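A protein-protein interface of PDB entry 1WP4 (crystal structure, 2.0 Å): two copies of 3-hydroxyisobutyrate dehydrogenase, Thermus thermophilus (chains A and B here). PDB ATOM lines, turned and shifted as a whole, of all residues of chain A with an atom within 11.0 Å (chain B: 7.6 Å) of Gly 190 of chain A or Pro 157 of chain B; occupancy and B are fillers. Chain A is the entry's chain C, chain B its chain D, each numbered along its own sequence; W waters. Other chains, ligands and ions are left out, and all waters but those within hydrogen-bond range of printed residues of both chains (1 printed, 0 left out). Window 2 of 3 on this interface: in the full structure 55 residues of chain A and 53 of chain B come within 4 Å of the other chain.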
ATOM      1  N   GLY A 182      -6.746  30.248 -10.439  1.00  0.00           N
ATOM      2  CA  GLY A 182      -6.591  28.825 -10.690  1.00  0.00           C
ATOM      3  C   GLY A 182      -7.083  28.383 -12.052  1.00  0.00           C
ATOM      4  O   GLY A 182      -6.415  27.612 -12.743  1.00  0.00           O
ATOM      5  N   LEU A 183      -8.255  28.865 -12.446  1.00  0.00           N
ATOM      6  CA  LEU A 183      -8.820  28.507 -13.740  1.00  0.00           C
ATOM      7  C   LEU A 183      -7.952  29.034 -14.876  1.00  0.00           C
ATOM      8  O   LEU A 183      -7.813  28.382 -15.909  1.00  0.00           O
ATOM      9  CB  LEU A 183     -10.244  29.057 -13.859  1.00  0.00           C
ATOM     10  CG  LEU A 183     -11.260  28.333 -12.967  1.00  0.00           C
ATOM     11  CD1 LEU A 183     -12.527  29.167 -12.834  1.00  0.00           C
ATOM     12  CD2 LEU A 183     -11.568  26.958 -13.557  1.00  0.00           C
ATOM     13  N   LEU A 184      -7.369  30.213 -14.679  1.00  0.00           N
ATOM     14  CA  LEU A 184      -6.506  30.817 -15.692  1.00  0.00           C
ATOM     15  C   LEU A 184      -5.340  29.871 -15.963  1.00  0.00           C
ATOM     16  O   LEU A 184      -5.036  29.553 -17.116  1.00  0.00           O
ATOM     17  CB  LEU A 184      -5.978  32.172 -15.198  1.00  0.00           C
ATOM     18  CG  LEU A 184      -5.160  33.090 -16.124  1.00  0.00           C
ATOM     19  CD1 LEU A 184      -3.819  32.460 -16.456  1.00  0.00           C
ATOM     20  CD2 LEU A 184      -5.944  33.379 -17.391  1.00  0.00           C
ATOM     21  N   ALA A 185      -4.693  29.419 -14.896  1.00  0.00           N
ATOM     22  CA  ALA A 185      -3.560  28.509 -15.017  1.00  0.00           C
ATOM     23  C   ALA A 185      -3.980  27.197 -15.678  1.00  0.00           C
ATOM     24  O   ALA A 185      -3.275  26.680 -16.545  1.00  0.00           O
ATOM     25  CB  ALA A 185      -2.958  28.237 -13.641  1.00  0.00           C
ATOM     26  N   LEU A 186      -5.130  26.662 -15.271  1.00  0.00           N
ATOM     27  CA  LEU A 186      -5.624  25.411 -15.839  1.00  0.00           C
ATOM     28  C   LEU A 186      -5.880  25.531 -17.339  1.00  0.00           C
ATOM     29  O   LEU A 186      -5.389  24.723 -18.132  1.00  0.00           O
ATOM     30  CB  LEU A 186      -6.910  24.975 -15.131  1.00  0.00           C
ATOM     31  CG  LEU A 186      -6.718  24.536 -13.675  1.00  0.00           C
ATOM     32  CD1 LEU A 186      -8.056  24.327 -13.006  1.00  0.00           C
ATOM     33  CD2 LEU A 186      -5.886  23.255 -13.646  1.00  0.00           C
ATOM     34  N   VAL A 187      -6.652  26.540 -17.726  1.00  0.00           N
ATOM     35  CA  VAL A 187      -6.963  26.744 -19.133  1.00  0.00           C
ATOM     36  C   VAL A 187      -5.673  26.912 -19.930  1.00  0.00           C
ATOM     37  O   VAL A 187      -5.533  26.376 -21.033  1.00  0.00           O
ATOM     38  CB  VAL A 187      -7.862  27.993 -19.329  1.00  0.00           C
ATOM     39  CG1 VAL A 187      -7.993  28.324 -20.808  1.00  0.00           C
ATOM     40  CG2 VAL A 187      -9.240  27.731 -18.736  1.00  0.00           C
ATOM     41  N   LYS A 188      -4.724  27.641 -19.358  1.00  0.00           N
ATOM     42  CA  LYS A 188      -3.461  27.889 -20.029  1.00  0.00           C
ATOM     43  C   LYS A 188      -2.724  26.603 -20.397  1.00  0.00           C
ATOM     44  O   LYS A 188      -1.999  26.570 -21.392  1.00  0.00           O
ATOM     45  CB  LYS A 188      -2.570  28.784 -19.165  1.00  0.00           C
ATOM     46  CG  LYS A 188      -1.509  29.533 -19.955  1.00  0.00           C
ATOM     47  CD  LYS A 188      -2.129  30.488 -20.976  1.00  0.00           C
ATOM     48  CE  LYS A 188      -1.047  31.155 -21.816  1.00  0.00           C
ATOM     49  NZ  LYS A 188      -1.590  32.125 -22.818  1.00  0.00           N
ATOM     50  N   GLN A 189      -2.889  25.540 -19.612  1.00  0.00           N
ATOM     51  CA  GLN A 189      -2.212  24.297 -19.966  1.00  0.00           C
ATOM     52  C   GLN A 189      -3.125  23.216 -20.533  1.00  0.00           C
ATOM     53  O   GLN A 189      -2.904  22.027 -20.319  1.00  0.00           O
ATOM     54  CB  GLN A 189      -1.380  23.744 -18.793  1.00  0.00           C
ATOM     55  CG  GLN A 189      -2.055  23.651 -17.441  1.00  0.00           C
ATOM     56  CD  GLN A 189      -1.087  23.154 -16.369  1.00  0.00           C
ATOM     57  OE1 GLN A 189      -1.064  21.970 -16.034  1.00  0.00           O
ATOM     58  NE2 GLN A 189      -0.265  24.060 -15.847  1.00  0.00           N
ATOM     59  N   GLY A 190      -4.159  23.645 -21.256  1.00  0.00           N
ATOM     60  CA  GLY A 190      -5.066  22.708 -21.900  1.00  0.00           C
ATOM     61  C   GLY A 190      -6.207  22.064 -21.136  1.00  0.00           C
ATOM     62  O   GLY A 190      -6.855  21.163 -21.663  1.00  0.00           O
ATOM     63  N   VAL A 191      -6.467  22.499 -19.910  1.00  0.00           N
ATOM     64  CA  VAL A 191      -7.559  21.919 -19.144  1.00  0.00           C
ATOM     65  C   VAL A 191      -8.877  22.588 -19.530  1.00  0.00           C
ATOM     66  O   VAL A 191      -8.922  23.797 -19.777  1.00  0.00           O
ATOM     67  CB  VAL A 191      -7.332  22.097 -17.626  1.00  0.00           C
ATOM     68  CG1 VAL A 191      -8.520  21.542 -16.845  1.00  0.00           C
ATOM     69  CG2 VAL A 191      -6.040  21.397 -17.211  1.00  0.00           C
ATOM     70  N   SER A 192      -9.943  21.799 -19.598  1.00  0.00           N
ATOM     71  CA  SER A 192     -11.260  22.335 -19.925  1.00  0.00           C
ATOM     72  C   SER A 192     -11.807  23.086 -18.716  1.00  0.00           C
ATOM     73  O   SER A 192     -11.955  22.511 -17.633  1.00  0.00           O
ATOM     74  CB  SER A 192     -12.221  21.201 -20.290  1.00  0.00           C
ATOM     75  OG  SER A 192     -13.560  21.669 -20.324  1.00  0.00           O
ATOM     76  N   ALA A 193     -12.109  24.368 -18.896  1.00  0.00           N
ATOM     77  CA  ALA A 193     -12.643  25.184 -17.807  1.00  0.00           C
ATOM     78  C   ALA A 193     -13.962  24.616 -17.286  1.00  0.00           C
ATOM     79  O   ALA A 193     -14.178  24.520 -16.077  1.00  0.00           O
ATOM     80  CB  ALA A 193     -12.844  26.625 -18.279  1.00  0.00           C
ATOM     81  N   GLU A 194     -14.846  24.243 -18.205  1.00  0.00           N
ATOM     82  CA  GLU A 194     -16.146  23.696 -17.832  1.00  0.00           C
ATOM     83  C   GLU A 194     -16.027  22.381 -17.060  1.00  0.00           C
ATOM     84  O   GLU A 194     -16.687  22.182 -16.041  1.00  0.00           O
ATOM     85  CB  GLU A 194     -16.998  23.474 -19.080  1.00  0.00           C
ATOM     86  CG  GLU A 194     -18.361  22.875 -18.791  1.00  0.00           C
ATOM     87  CD  GLU A 194     -19.171  22.651 -20.050  1.00  0.00           C
ATOM     88  OE1 GLU A 194     -18.686  21.935 -20.950  1.00  0.00           O
ATOM     89  OE2 GLU A 194     -20.293  23.191 -20.138  1.00  0.00           O
ATOM     90  N   LYS A 195     -15.186  21.482 -17.556  1.00  0.00           N
ATOM     91  CA  LYS A 195     -14.995  20.192 -16.913  1.00  0.00           C
ATOM     92  C   LYS A 195     -14.292  20.341 -15.569  1.00  0.00           C
ATOM     93  O   LYS A 195     -14.590  19.611 -14.630  1.00  0.00           O
ATOM     94  CB  LYS A 195     -14.211  19.258 -17.840  1.00  0.00           C
ATOM     95  CG  LYS A 195     -15.015  18.788 -19.056  1.00  0.00           C
ATOM     96  CD  LYS A 195     -16.200  17.926 -18.621  1.00  0.00           C
ATOM     97  CE  LYS A 195     -16.969  17.348 -19.803  1.00  0.00           C
ATOM     98  NZ  LYS A 195     -17.714  18.381 -20.571  1.00  0.00           N
ATOM     99  N   ALA A 196     -13.367  21.291 -15.478  1.00  0.00           N
ATOM    100  CA  ALA A 196     -12.655  21.543 -14.227  1.00  0.00           C
ATOM    101  C   ALA A 196     -13.653  22.036 -13.176  1.00  0.00           C
ATOM    102  O   ALA A 196     -13.623  21.616 -12.017  1.00  0.00           O
ATOM    103  CB  ALA A 196     -11.561  22.587 -14.445  1.00  0.00           C
ATOM    104  N   VAL A 286      -5.472  34.960 -22.297  1.00  0.00           N
ATOM    105  CA  VAL A 286      -6.399  33.878 -22.616  1.00  0.00           C
ATOM    106  C   VAL A 286      -7.702  34.065 -21.846  1.00  0.00           C
ATOM    107  O   VAL A 286      -7.713  34.617 -20.747  1.00  0.00           O
ATOM    108  CB  VAL A 286      -5.797  32.493 -22.259  1.00  0.00           C
ATOM    109  CG1 VAL A 286      -5.746  32.312 -20.746  1.00  0.00           C
ATOM    110  CG2 VAL A 286      -6.614  31.391 -22.897  1.00  0.00           C
ATOM    111  N   GLU A 287      -8.802  33.608 -22.431  1.00  0.00           N
ATOM    112  CA  GLU A 287     -10.095  33.730 -21.787  1.00  0.00           C
ATOM    113  C   GLU A 287     -10.403  32.488 -20.973  1.00  0.00           C
ATOM    114  O   GLU A 287      -9.977  31.387 -21.313  1.00  0.00           O
ATOM    115  CB  GLU A 287     -11.189  33.932 -22.833  1.00  0.00           C
ATOM    116  CG  GLU A 287     -11.097  35.249 -23.577  1.00  0.00           C
ATOM    117  CD  GLU A 287     -12.161  35.373 -24.642  1.00  0.00           C
ATOM    118  OE1 GLU A 287     -12.361  36.494 -25.154  1.00  0.00           O
ATOM    119  OE2 GLU A 287     -12.795  34.345 -24.967  1.00  0.00           O
ATOM    120  N   ARG A 289     -12.764  29.965 -20.374  1.00  0.00           N
ATOM    121  CA  ARG A 289     -13.942  29.316 -20.938  1.00  0.00           C
ATOM    122  C   ARG A 289     -13.571  28.049 -21.690  1.00  0.00           C
ATOM    123  O   ARG A 289     -12.365  27.834 -21.917  1.00  0.00           O
ATOM    124  CB  ARG A 289     -14.691  30.253 -21.890  1.00  0.00           C
ATOM    125  CG  ARG A 289     -13.958  30.597 -23.173  1.00  0.00           C
ATOM    126  CD  ARG A 289     -14.976  30.921 -24.259  1.00  0.00           C
ATOM    127  NE  ARG A 289     -14.490  31.898 -25.227  1.00  0.00           N
ATOM    128  CZ  ARG A 289     -15.233  32.406 -26.208  1.00  0.00           C
ATOM    129  NH1 ARG A 289     -16.497  32.029 -26.354  1.00  0.00           N
ATOM    130  NH2 ARG A 289     -14.718  33.305 -27.035  1.00  0.00           N
ATOM    131  OXT ARG A 289     -14.496  27.296 -22.048  1.00  0.00           O
ATOM    132  N   ARG B  98       3.324  13.535 -17.058  1.00  0.00           N
ATOM    133  CA  ARG B  98       3.299  13.501 -18.520  1.00  0.00           C
ATOM    134  C   ARG B  98       4.530  12.753 -19.023  1.00  0.00           C
ATOM    135  O   ARG B  98       4.457  11.979 -19.978  1.00  0.00           O
ATOM    136  CB  ARG B  98       3.286  14.922 -19.099  1.00  0.00           C
ATOM    137  CG  ARG B  98       2.040  15.717 -18.755  1.00  0.00           C
ATOM    138  CD  ARG B  98       1.946  16.996 -19.573  1.00  0.00           C
ATOM    139  NE  ARG B  98       0.825  17.824 -19.137  1.00  0.00           N
ATOM    140  CZ  ARG B  98       0.892  18.735 -18.168  1.00  0.00           C
ATOM    141  NH1 ARG B  98       2.034  18.948 -17.529  1.00  0.00           N
ATOM    142  NH2 ARG B  98      -0.191  19.426 -17.831  1.00  0.00           N
ATOM    143  N   TYR B 111      -1.272   5.499 -19.982  1.00  0.00           N
ATOM    144  CA  TYR B 111      -1.393   6.145 -18.681  1.00  0.00           C
ATOM    145  C   TYR B 111      -2.458   7.239 -18.665  1.00  0.00           C
ATOM    146  O   TYR B 111      -2.589   8.010 -19.617  1.00  0.00           O
ATOM    147  CB  TYR B 111      -0.044   6.769 -18.289  1.00  0.00           C
ATOM    148  CG  TYR B 111      -0.054   7.554 -16.992  1.00  0.00           C
ATOM    149  CD1 TYR B 111       0.285   6.945 -15.781  1.00  0.00           C
ATOM    150  CD2 TYR B 111      -0.399   8.910 -16.974  1.00  0.00           C
ATOM    151  CE1 TYR B 111       0.284   7.664 -14.588  1.00  0.00           C
ATOM    152  CE2 TYR B 111      -0.408   9.640 -15.780  1.00  0.00           C
ATOM    153  CZ  TYR B 111      -0.062   9.010 -14.594  1.00  0.00           C
ATOM    154  OH  TYR B 111      -0.046   9.721 -13.417  1.00  0.00           O
ATOM    155  N   LEU B 112      -3.209   7.296 -17.573  1.00  0.00           N
ATOM    156  CA  LEU B 112      -4.235   8.311 -17.382  1.00  0.00           C
ATOM    157  C   LEU B 112      -4.168   8.778 -15.935  1.00  0.00           C
ATOM    158  O   LEU B 112      -4.241   7.951 -15.016  1.00  0.00           O
ATOM    159  CB  LEU B 112      -5.633   7.743 -17.637  1.00  0.00           C
ATOM    160  CG  LEU B 112      -5.977   7.194 -19.022  1.00  0.00           C
ATOM    161  CD1 LEU B 112      -7.445   6.793 -19.054  1.00  0.00           C
ATOM    162  CD2 LEU B 112      -5.708   8.254 -20.071  1.00  0.00           C
ATOM    163  N   ASP B 113      -3.998  10.079 -15.707  1.00  0.00           N
ATOM    164  CA  ASP B 113      -3.997  10.527 -14.326  1.00  0.00           C
ATOM    165  C   ASP B 113      -5.458  10.543 -13.914  1.00  0.00           C
ATOM    166  O   ASP B 113      -6.328  10.947 -14.695  1.00  0.00           O
ATOM    167  CB  ASP B 113      -3.339  11.910 -14.128  1.00  0.00           C
ATOM    168  CG  ASP B 113      -3.603  12.888 -15.258  1.00  0.00           C
ATOM    169  OD1 ASP B 113      -3.804  14.086 -14.946  1.00  0.00           O
ATOM    170  OD2 ASP B 113      -3.577  12.488 -16.441  1.00  0.00           O
ATOM    171  N   LEU B 132     -10.285  12.664 -14.692  1.00  0.00           N
ATOM    172  CA  LEU B 132      -9.416  11.992 -15.652  1.00  0.00           C
ATOM    173  C   LEU B 132      -8.666  12.880 -16.633  1.00  0.00           C
ATOM    174  O   LEU B 132      -9.212  13.841 -17.172  1.00  0.00           O
ATOM    175  CB  LEU B 132     -10.220  10.968 -16.464  1.00  0.00           C
ATOM    176  CG  LEU B 132     -10.751   9.714 -15.770  1.00  0.00           C
ATOM    177  CD1 LEU B 132     -11.679   8.957 -16.720  1.00  0.00           C
ATOM    178  CD2 LEU B 132      -9.589   8.835 -15.355  1.00  0.00           C
ATOM    179  N   GLY B 133      -7.408  12.522 -16.866  1.00  0.00           N
ATOM    180  CA  GLY B 133      -6.577  13.239 -17.811  1.00  0.00           C
ATOM    181  C   GLY B 133      -6.024  12.202 -18.773  1.00  0.00           C
ATOM    182  O   GLY B 133      -5.454  11.198 -18.337  1.00  0.00           O
ATOM    183  N   GLY B 134      -6.197  12.419 -20.073  1.00  0.00           N
ATOM    184  CA  GLY B 134      -5.696  11.461 -21.044  1.00  0.00           C
ATOM    185  C   GLY B 134      -6.472  11.444 -22.348  1.00  0.00           C
ATOM    186  O   GLY B 134      -7.391  12.240 -22.528  1.00  0.00           O
ATOM    187  N   PRO B 135      -6.122  10.543 -23.282  1.00  0.00           N
ATOM    188  CA  PRO B 135      -6.768  10.393 -24.588  1.00  0.00           C
ATOM    189  C   PRO B 135      -8.254   9.982 -24.456  1.00  0.00           C
ATOM    190  O   PRO B 135      -8.640   9.200 -23.601  1.00  0.00           O
ATOM    191  CB  PRO B 135      -5.967   9.360 -25.389  1.00  0.00           C
ATOM    192  CG  PRO B 135      -4.584   9.288 -24.742  1.00  0.00           C
ATOM    193  CD  PRO B 135      -4.979   9.639 -23.228  1.00  0.00           C
ATOM    194  N   GLU B 136      -9.102  10.605 -25.317  1.00  0.00           N
ATOM    195  CA  GLU B 136     -10.550  10.365 -25.240  1.00  0.00           C
ATOM    196  C   GLU B 136     -10.828   8.860 -25.243  1.00  0.00           C
ATOM    197  O   GLU B 136     -11.491   8.323 -24.366  1.00  0.00           O
ATOM    198  CB  GLU B 136     -11.228  11.102 -26.409  1.00  0.00           C
ATOM    199  CG  GLU B 136     -12.707  10.730 -26.574  1.00  0.00           C
ATOM    200  CD  GLU B 136     -13.376  11.674 -27.554  1.00  0.00           C
ATOM    201  OE1 GLU B 136     -12.896  11.795 -28.672  1.00  0.00           O
ATOM    202  OE2 GLU B 136     -14.423  12.222 -27.218  1.00  0.00           O
ATOM    203  N   HIS B 154     -13.847  13.804 -17.471  1.00  0.00           N
ATOM    204  CA  HIS B 154     -12.651  13.873 -18.305  1.00  0.00           C
ATOM    205  C   HIS B 154     -12.337  15.365 -18.422  1.00  0.00           C
ATOM    206  O   HIS B 154     -13.042  16.095 -19.114  1.00  0.00           O
ATOM    207  CB  HIS B 154     -12.932  13.286 -19.690  1.00  0.00           C
ATOM    208  CG  HIS B 154     -11.737  13.271 -20.592  1.00  0.00           C
ATOM    209  ND1 HIS B 154     -11.831  13.041 -21.947  1.00  0.00           N
ATOM    210  CD2 HIS B 154     -10.420  13.451 -20.332  1.00  0.00           C
ATOM    211  CE1 HIS B 154     -10.624  13.079 -22.484  1.00  0.00           C
ATOM    212  NE2 HIS B 154      -9.750  13.326 -21.525  1.00  0.00           N
ATOM    213  N   VAL B 155     -11.278  15.812 -17.751  1.00  0.00           N
ATOM    214  CA  VAL B 155     -10.927  17.231 -17.744  1.00  0.00           C
ATOM    215  C   VAL B 155      -9.891  17.715 -18.754  1.00  0.00           C
ATOM    216  O   VAL B 155      -9.691  18.921 -18.897  1.00  0.00           O
ATOM    217  CB  VAL B 155     -10.458  17.663 -16.334  1.00  0.00           C
ATOM    218  CG1 VAL B 155     -11.597  17.506 -15.339  1.00  0.00           C
ATOM    219  CG2 VAL B 155      -9.257  16.834 -15.907  1.00  0.00           C
ATOM    220  N   GLY B 156      -9.235  16.790 -19.448  1.00  0.00           N
ATOM    221  CA  GLY B 156      -8.236  17.185 -20.427  1.00  0.00           C
ATOM    222  C   GLY B 156      -7.200  16.110 -20.705  1.00  0.00           C
ATOM    223  O   GLY B 156      -7.391  14.957 -20.319  1.00  0.00           O
ATOM    224  N   PRO B 157      -6.096  16.450 -21.390  1.00  0.00           N
ATOM    225  CA  PRO B 157      -5.052  15.464 -21.694  1.00  0.00           C
ATOM    226  C   PRO B 157      -4.283  15.055 -20.439  1.00  0.00           C
ATOM    227  O   PRO B 157      -4.554  15.562 -19.353  1.00  0.00           O
ATOM    228  CB  PRO B 157      -4.181  16.185 -22.725  1.00  0.00           C
ATOM    229  CG  PRO B 157      -4.333  17.637 -22.342  1.00  0.00           C
ATOM    230  CD  PRO B 157      -5.809  17.748 -22.029  1.00  0.00           C
ATOM    231  N   VAL B 158      -3.333  14.134 -20.586  1.00  0.00           N
ATOM    232  CA  VAL B 158      -2.553  13.666 -19.449  1.00  0.00           C
ATOM    233  C   VAL B 158      -1.984  14.821 -18.638  1.00  0.00           C
ATOM    234  O   VAL B 158      -1.386  15.751 -19.188  1.00  0.00           O
ATOM    235  CB  VAL B 158      -1.386  12.755 -19.893  1.00  0.00           C
ATOM    236  CG1 VAL B 158      -0.527  12.386 -18.687  1.00  0.00           C
ATOM    237  CG2 VAL B 158      -1.930  11.499 -20.551  1.00  0.00           C
ATOM    238  N   GLY B 159      -2.174  14.752 -17.324  1.00  0.00           N
ATOM    239  CA  GLY B 159      -1.681  15.800 -16.452  1.00  0.00           C
ATOM    240  C   GLY B 159      -2.764  16.773 -16.029  1.00  0.00           C
ATOM    241  O   GLY B 159      -2.623  17.466 -15.025  1.00  0.00           O
ATOM    242  N   ALA B 160      -3.854  16.823 -16.790  1.00  0.00           N
ATOM    243  CA  ALA B 160      -4.954  17.730 -16.480  1.00  0.00           C
ATOM    244  C   ALA B 160      -5.673  17.296 -15.206  1.00  0.00           C
ATOM    245  O   ALA B 160      -6.114  18.135 -14.421  1.00  0.00           O
ATOM    246  CB  ALA B 160      -5.930  17.785 -17.648  1.00  0.00           C
ATOM    247  N   GLY B 161      -5.795  15.985 -15.008  1.00  0.00           N
ATOM    248  CA  GLY B 161      -6.447  15.480 -13.809  1.00  0.00           C
ATOM    249  C   GLY B 161      -5.694  15.914 -12.561  1.00  0.00           C
ATOM    250  O   GLY B 161      -6.290  16.446 -11.620  1.00  0.00           O
ATOM    251  N   HIS B 162      -4.381  15.693 -12.553  1.00  0.00           N
ATOM    252  CA  HIS B 162      -3.551  16.081 -11.416  1.00  0.00           C
ATOM    253  C   HIS B 162      -3.614  17.581 -11.163  1.00  0.00           C
ATOM    254  O   HIS B 162      -3.640  18.016 -10.016  1.00  0.00           O
ATOM    255  CB  HIS B 162      -2.090  15.677 -11.637  1.00  0.00           C
ATOM    256  CG  HIS B 162      -1.865  14.197 -11.674  1.00  0.00           C
ATOM    257  ND1 HIS B 162      -2.447  13.332 -10.770  1.00  0.00           N
ATOM    258  CD2 HIS B 162      -1.084  13.435 -12.475  1.00  0.00           C
ATOM    259  CE1 HIS B 162      -2.033  12.101 -11.014  1.00  0.00           C
ATOM    260  NE2 HIS B 162      -1.205  12.135 -12.043  1.00  0.00           N
HETATM  261  O   HOH W   1      -2.374  20.155 -16.974  1.00  0.00           O
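Of the 18 printed residues of chain A, 5 touch a printed residue of chain B. Hydrophobic or aromatic side chains of chain A that line the printed part of chain B: Val 191. Of the 18 printed residues of chain B, 5 touch a printed residue of chain A. Hydrophobic or aromatic side chains of chain B within 4 Å of the printed part of chain A: Val 155, Pro 157 and Ala 160. Along chain B the printed residues that touch a printed residue of chain A span positions 98 to 160. Among the printed residues, no Asp or Glu carboxylate lies within 4 Å of a Lys or Arg side-chain nitrogen of the other chain.
CD of Pro 157 of chain B touches O of Gly 190 of chain A, 3.6 Å away. Val 155 of chain B touches Val 191 of chain A. Val 191 of chain A touches Ala 160 of chain B (CG2 to CB, 3.6 Å). Lys 195 of chain A touches His 154 of chain B. Lys 195 of chain A touches Val 155 of chain B (O to CG1, 3.7 Å).
Of the printed residues of chain B, Gly 190 of chain A touches Pro 157 (3.6 Å). Pro 157 of chain B touches just one residue of chain A: Gly 190. No residue of chain A comes within 4 Å of Gly 134 of chain B. No residue of chain A comes within 4 Å of Gly 156 of chain B. No residue of chain A comes within 4 Å of Val 158 of chain B. No residue of chain A comes within 4 Å of Gly 159 of chain B. Ala 160 of chain B touches just one residue of chain A: Val 191 (3.6 Å). Printed residues of chain A within 4 Å of Arg 98 of chain B: Gln 189. Of the printed residues of chain B, Lys 195 of chain A touches His 154 (3.3 Å) and Val 155 (3.7 Å). Printed residues of chain B within 4 Å of Ser 192 of chain A: Val 155 (3.0 Å). Printed residues of chain B within 4 Å of Val 191 of chain A: Val 155 (3.5 Å) and Ala 160 (3.6 Å). The nearest residue of chain B that does not touch Gly 190 of chain A is Gly 156 of chain B (4.4 Å).
Water W1 lies within hydrogen-bond range of OE1 of Gln 189 of chain A, NH2 of Arg 98 of chain B and O of Gly 159 of chain B.
O of Leu 186 of chain A is in hydrogen-bond range of N of Val 191 of chain A. OG of Ser 192 of chain A sits at hydrogen-bond distance from N of Lys 195 of chain A (3.2 Å). The backbone carbonyl oxygen (O) of Val 158 of chain B lies within hydrogen-bond range of the guanidinium group (NE) of Arg 98 of chain B (3.0 Å). The backbone NH (N) of Val 155 of chain B lies within hydrogen-bond range of the backbone carbonyl oxygen (O) of Leu 132 of chain B (2.9 Å). NE2 of His 154 of chain B is in hydrogen-bond range of O of Gly 134 of chain B, 2.8 Å away. The backbone carbonyl oxygen (O) of Gly 156 of chain B is in hydrogen-bond range of a ring nitrogen (NE2) of His 154 of chain B.
The side-chain amide oxygen (OE1) of Gln 189 of chain A is in hydrogen-bond range of the guanidinium group (NH2) of Arg 98 of chain B. The backbone carbonyl oxygen (O) of Val 155 of chain B lies within hydrogen-bond range of the backbone NH (N) of Ser 192 of chain A.
No position is printed for both chains. Of the 7 pairs that touch across the chains among the printed residues, none has its exchanged pair printed and touching as well.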
